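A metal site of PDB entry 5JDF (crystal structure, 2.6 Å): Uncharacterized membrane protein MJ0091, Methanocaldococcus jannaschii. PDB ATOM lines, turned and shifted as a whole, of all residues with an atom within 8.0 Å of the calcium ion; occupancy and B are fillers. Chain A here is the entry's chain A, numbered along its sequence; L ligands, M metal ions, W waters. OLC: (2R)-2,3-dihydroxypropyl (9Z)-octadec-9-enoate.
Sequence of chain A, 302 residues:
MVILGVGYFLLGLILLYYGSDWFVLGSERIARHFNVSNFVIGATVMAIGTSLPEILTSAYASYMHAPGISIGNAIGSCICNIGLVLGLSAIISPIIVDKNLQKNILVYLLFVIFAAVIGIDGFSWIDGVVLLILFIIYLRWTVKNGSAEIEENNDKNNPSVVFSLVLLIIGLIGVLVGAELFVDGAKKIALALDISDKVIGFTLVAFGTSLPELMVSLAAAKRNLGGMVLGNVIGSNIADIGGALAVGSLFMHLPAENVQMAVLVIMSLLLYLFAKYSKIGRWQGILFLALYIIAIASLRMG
Water W1 bridges OD2 of Asp 121 and OG of Ser 124.
Four residues have an atom within 4 Å of the calcium ion: Ile 118, Asp 121, Gly 122 and Asp 127. The nearest printed residue that does not touch the calcium ion is Phe 123 (4.2 Å).
The calcium ion is bound by O of Ile 118 (2.4 Å). Water W1 binds the calcium ion (2.4 Å). O of Gly 122 is bound to the calcium ion, at 2.4 Å. OD2 of Asp 127 is bound to the calcium ion (2.5 Å). The side-chain carboxylate (OD1) of Asp 121 is bound to the calcium ion, at 2.6 Å. O25 of the ligand is bound to the calcium ion (2.8 Å). The calcium ion has six donor atoms within binding distance.
N of Asp 127 lies within hydrogen-bond range of OG of Ser 124 (3.2 Å). NE2 of His 253 is in hydrogen-bond range of O of Asp 121.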
ATOM      1  N   ALA A 115     -12.971  23.922   9.686  1.00  0.00           N
ATOM      2  CA  ALA A 115     -13.878  24.062   8.554  1.00  0.00           C
ATOM      3  C   ALA A 115     -13.378  25.111   7.577  1.00  0.00           C
ATOM      4  O   ALA A 115     -13.465  24.939   6.356  1.00  0.00           O
ATOM      5  CB  ALA A 115     -15.275  24.415   9.035  1.00  0.00           C
ATOM      6  N   ALA A 116     -12.833  26.201   8.118  1.00  0.00           N
ATOM      7  CA  ALA A 116     -12.343  27.306   7.308  1.00  0.00           C
ATOM      8  C   ALA A 116     -11.148  26.888   6.458  1.00  0.00           C
ATOM      9  O   ALA A 116     -11.033  27.291   5.300  1.00  0.00           O
ATOM     10  CB  ALA A 116     -11.987  28.479   8.194  1.00  0.00           C
ATOM     11  N   VAL A 117     -10.258  26.083   7.044  1.00  0.00           N
ATOM     12  CA  VAL A 117      -9.065  25.637   6.346  1.00  0.00           C
ATOM     13  C   VAL A 117      -9.388  24.711   5.175  1.00  0.00           C
ATOM     14  O   VAL A 117      -8.896  24.901   4.062  1.00  0.00           O
ATOM     15  CB  VAL A 117      -8.104  24.903   7.306  1.00  0.00           C
ATOM     16  CG1 VAL A 117      -7.003  24.198   6.535  1.00  0.00           C
ATOM     17  CG2 VAL A 117      -7.510  25.880   8.323  1.00  0.00           C
ATOM     18  N   ILE A 118     -10.241  23.719   5.423  1.00  0.00           N
ATOM     19  CA  ILE A 118     -10.592  22.746   4.396  1.00  0.00           C
ATOM     20  C   ILE A 118     -11.564  23.324   3.374  1.00  0.00           C
ATOM     21  O   ILE A 118     -11.902  22.676   2.390  1.00  0.00           O
ATOM     22  CB  ILE A 118     -11.213  21.469   5.010  1.00  0.00           C
ATOM     23  CG1 ILE A 118     -12.625  21.753   5.516  1.00  0.00           C
ATOM     24  CG2 ILE A 118     -10.323  20.927   6.114  1.00  0.00           C
ATOM     25  CD1 ILE A 118     -13.368  20.522   5.972  1.00  0.00           C
ATOM     26  N   GLY A 119     -12.014  24.554   3.610  1.00  0.00           N
ATOM     27  CA  GLY A 119     -12.969  25.197   2.734  1.00  0.00           C
ATOM     28  C   GLY A 119     -12.375  26.228   1.793  1.00  0.00           C
ATOM     29  O   GLY A 119     -13.067  26.798   0.961  1.00  0.00           O
ATOM     30  N   ILE A 120     -11.067  26.462   1.937  1.00  0.00           N
ATOM     31  CA  ILE A 120     -10.346  27.427   1.114  1.00  0.00           C
ATOM     32  C   ILE A 120     -10.498  27.125  -0.377  1.00  0.00           C
ATOM     33  O   ILE A 120     -10.672  28.032  -1.189  1.00  0.00           O
ATOM     34  CB  ILE A 120      -8.849  27.439   1.472  1.00  0.00           C
ATOM     35  CG1 ILE A 120      -8.656  27.830   2.937  1.00  0.00           C
ATOM     36  CG2 ILE A 120      -8.091  28.404   0.568  1.00  0.00           C
ATOM     37  CD1 ILE A 120      -7.211  27.795   3.389  1.00  0.00           C
ATOM     38  N   ASP A 121     -10.433  25.848  -0.724  1.00  0.00           N
ATOM     39  CA  ASP A 121     -10.606  25.415  -2.107  1.00  0.00           C
ATOM     40  C   ASP A 121     -12.040  24.982  -2.355  1.00  0.00           C
ATOM     41  O   ASP A 121     -12.333  24.297  -3.339  1.00  0.00           O
ATOM     42  CB  ASP A 121      -9.640  24.273  -2.439  1.00  0.00           C
ATOM     43  CG  ASP A 121      -9.696  23.152  -1.415  1.00  0.00           C
ATOM     44  OD1 ASP A 121     -10.023  23.429  -0.244  1.00  0.00           O
ATOM     45  OD2 ASP A 121      -9.400  22.000  -1.789  1.00  0.00           O
ATOM     46  N   GLY A 122     -12.939  25.382  -1.466  1.00  0.00           N
ATOM     47  CA  GLY A 122     -14.327  24.993  -1.548  1.00  0.00           C
ATOM     48  C   GLY A 122     -14.639  23.829  -0.622  1.00  0.00           C
ATOM     49  O   GLY A 122     -13.785  23.423   0.165  1.00  0.00           O
ATOM     50  N   PHE A 123     -15.850  23.302  -0.714  1.00  0.00           N
ATOM     51  CA  PHE A 123     -16.256  22.175   0.113  1.00  0.00           C
ATOM     52  C   PHE A 123     -16.698  20.984  -0.728  1.00  0.00           C
ATOM     53  O   PHE A 123     -17.813  20.975  -1.262  1.00  0.00           O
ATOM     54  CB  PHE A 123     -17.373  22.573   1.082  1.00  0.00           C
ATOM     55  CG  PHE A 123     -16.919  23.481   2.188  1.00  0.00           C
ATOM     56  CD1 PHE A 123     -16.341  22.955   3.333  1.00  0.00           C
ATOM     57  CD2 PHE A 123     -17.088  24.852   2.093  1.00  0.00           C
ATOM     58  CE1 PHE A 123     -15.940  23.788   4.356  1.00  0.00           C
ATOM     59  CE2 PHE A 123     -16.678  25.688   3.115  1.00  0.00           C
ATOM     60  CZ  PHE A 123     -16.097  25.153   4.251  1.00  0.00           C
ATOM     61  N   SER A 124     -15.819  19.999  -0.854  1.00  0.00           N
ATOM     62  CA  SER A 124     -16.153  18.766  -1.557  1.00  0.00           C
ATOM     63  C   SER A 124     -17.131  17.953  -0.742  1.00  0.00           C
ATOM     64  O   SER A 124     -17.349  18.227   0.446  1.00  0.00           O
ATOM     65  CB  SER A 124     -14.887  17.948  -1.848  1.00  0.00           C
ATOM     66  OG  SER A 124     -14.289  17.496  -0.647  1.00  0.00           O
ATOM     67  N   TRP A 125     -17.742  16.943  -1.365  1.00  0.00           N
ATOM     68  CA  TRP A 125     -18.660  16.062  -0.659  1.00  0.00           C
ATOM     69  C   TRP A 125     -17.936  15.334   0.471  1.00  0.00           C
ATOM     70  O   TRP A 125     -18.533  15.006   1.486  1.00  0.00           O
ATOM     71  CB  TRP A 125     -19.292  15.053  -1.622  1.00  0.00           C
ATOM     72  CG  TRP A 125     -18.300  14.163  -2.299  1.00  0.00           C
ATOM     73  CD1 TRP A 125     -17.625  14.428  -3.453  1.00  0.00           C
ATOM     74  CD2 TRP A 125     -17.871  12.866  -1.868  1.00  0.00           C
ATOM     75  NE1 TRP A 125     -16.797  13.376  -3.764  1.00  0.00           N
ATOM     76  CE2 TRP A 125     -16.932  12.405  -2.805  1.00  0.00           C
ATOM     77  CE3 TRP A 125     -18.197  12.064  -0.770  1.00  0.00           C
ATOM     78  CZ2 TRP A 125     -16.318  11.163  -2.686  1.00  0.00           C
ATOM     79  CZ3 TRP A 125     -17.574  10.826  -0.651  1.00  0.00           C
ATOM     80  CH2 TRP A 125     -16.646  10.392  -1.610  1.00  0.00           C
ATOM     81  N   ILE A 126     -16.640  15.104   0.279  1.00  0.00           N
ATOM     82  CA  ILE A 126     -15.803  14.487   1.298  1.00  0.00           C
ATOM     83  C   ILE A 126     -15.634  15.433   2.494  1.00  0.00           C
ATOM     84  O   ILE A 126     -15.691  14.987   3.643  1.00  0.00           O
ATOM     85  CB  ILE A 126     -14.416  14.117   0.738  1.00  0.00           C
ATOM     86  CG1 ILE A 126     -14.549  13.008  -0.311  1.00  0.00           C
ATOM     87  CG2 ILE A 126     -13.480  13.657   1.855  1.00  0.00           C
ATOM     88  CD1 ILE A 126     -13.237  12.496  -0.840  1.00  0.00           C
ATOM     89  N   ASP A 127     -15.442  16.716   2.219  1.00  0.00           N
ATOM     90  CA  ASP A 127     -15.370  17.728   3.265  1.00  0.00           C
ATOM     91  C   ASP A 127     -16.624  17.689   4.122  1.00  0.00           C
ATOM     92  O   ASP A 127     -16.554  17.792   5.346  1.00  0.00           O
ATOM     93  CB  ASP A 127     -15.185  19.125   2.673  1.00  0.00           C
ATOM     94  CG  ASP A 127     -13.809  19.345   2.083  1.00  0.00           C
ATOM     95  OD1 ASP A 127     -12.890  18.563   2.416  1.00  0.00           O
ATOM     96  OD2 ASP A 127     -13.647  20.301   1.305  1.00  0.00           O
ATOM     97  N   GLY A 128     -17.766  17.528   3.466  1.00  0.00           N
ATOM     98  CA  GLY A 128     -19.042  17.464   4.155  1.00  0.00           C
ATOM     99  C   GLY A 128     -19.188  16.242   5.037  1.00  0.00           C
ATOM    100  O   GLY A 128     -19.735  16.319   6.128  1.00  0.00           O
ATOM    101  N   HIS A 253     -20.368  20.406  -5.164  1.00  0.00           N
ATOM    102  CA  HIS A 253     -19.260  21.147  -4.598  1.00  0.00           C
ATOM    103  C   HIS A 253     -19.659  22.579  -4.265  1.00  0.00           C
ATOM    104  O   HIS A 253     -20.236  23.276  -5.089  1.00  0.00           O
ATOM    105  CB  HIS A 253     -18.063  21.151  -5.560  1.00  0.00           C
ATOM    106  CG  HIS A 253     -16.863  21.871  -5.017  1.00  0.00           C
ATOM    107  ND1 HIS A 253     -15.913  21.254  -4.253  1.00  0.00           N
ATOM    108  CD2 HIS A 253     -16.475  23.167  -5.151  1.00  0.00           C
ATOM    109  CE1 HIS A 253     -14.977  22.137  -3.927  1.00  0.00           C
ATOM    110  NE2 HIS A 253     -15.295  23.290  -4.455  1.00  0.00           N
ATOM    111  N   LEU A 254     -19.362  22.998  -3.037  1.00  0.00           N
ATOM    112  CA  LEU A 254     -19.682  24.346  -2.593  1.00  0.00           C
ATOM    113  C   LEU A 254     -18.529  25.296  -2.881  1.00  0.00           C
ATOM    114  O   LEU A 254     -17.378  24.990  -2.562  1.00  0.00           O
ATOM    115  CB  LEU A 254     -20.023  24.363  -1.106  1.00  0.00           C
ATOM    116  CG  LEU A 254     -21.117  23.400  -0.629  1.00  0.00           C
ATOM    117  CD1 LEU A 254     -21.357  23.581   0.865  1.00  0.00           C
ATOM    118  CD2 LEU A 254     -22.403  23.618  -1.408  1.00  0.00           C
ATOM    119  N   ALA A 256     -15.926  28.409  -2.572  1.00  0.00           N
ATOM    120  CA  ALA A 256     -15.207  28.915  -1.405  1.00  0.00           C
ATOM    121  C   ALA A 256     -15.671  30.306  -0.988  1.00  0.00           C
ATOM    122  O   ALA A 256     -15.703  31.232  -1.806  1.00  0.00           O
ATOM    123  CB  ALA A 256     -13.706  28.927  -1.679  1.00  0.00           C
HETATM  124  C8  OLC L   1      -6.331  22.575  12.725  1.00  0.00           C
HETATM  125  C24 OLC L   1      -9.700  19.940   2.100  1.00  0.00           C
HETATM  126  C7  OLC L   1      -6.299  22.732  11.203  1.00  0.00           C
HETATM  127  C6  OLC L   1      -6.361  21.344  10.536  1.00  0.00           C
HETATM  128  C5  OLC L   1      -6.327  21.556   9.020  1.00  0.00           C
HETATM  129  C4  OLC L   1      -6.392  20.217   8.271  1.00  0.00           C
HETATM  130  C3  OLC L   1      -6.356  20.547   6.779  1.00  0.00           C
HETATM  131  C2  OLC L   1      -6.424  19.288   5.916  1.00  0.00           C
HETATM  132  C21 OLC L   1      -7.222  19.749   2.337  1.00  0.00           C
HETATM  133  C1  OLC L   1      -6.387  19.736   4.447  1.00  0.00           C
HETATM  134  C22 OLC L   1      -8.431  19.354   1.476  1.00  0.00           C
HETATM  135  O19 OLC L   1      -5.520  20.515   4.060  1.00  0.00           O
HETATM  136  O25 OLC L   1     -10.831  19.575   1.305  1.00  0.00           O
HETATM  137  O23 OLC L   1      -8.263  19.877   0.159  1.00  0.00           O
HETATM  138  O20 OLC L   1      -7.381  19.230   3.664  1.00  0.00           O
HETATM  139 CA    CA M   1     -11.987  21.796   0.165  1.00  0.00          CA
HETATM  140  O   HOH W   1     -12.240  20.160  -1.593  1.00  0.00           O
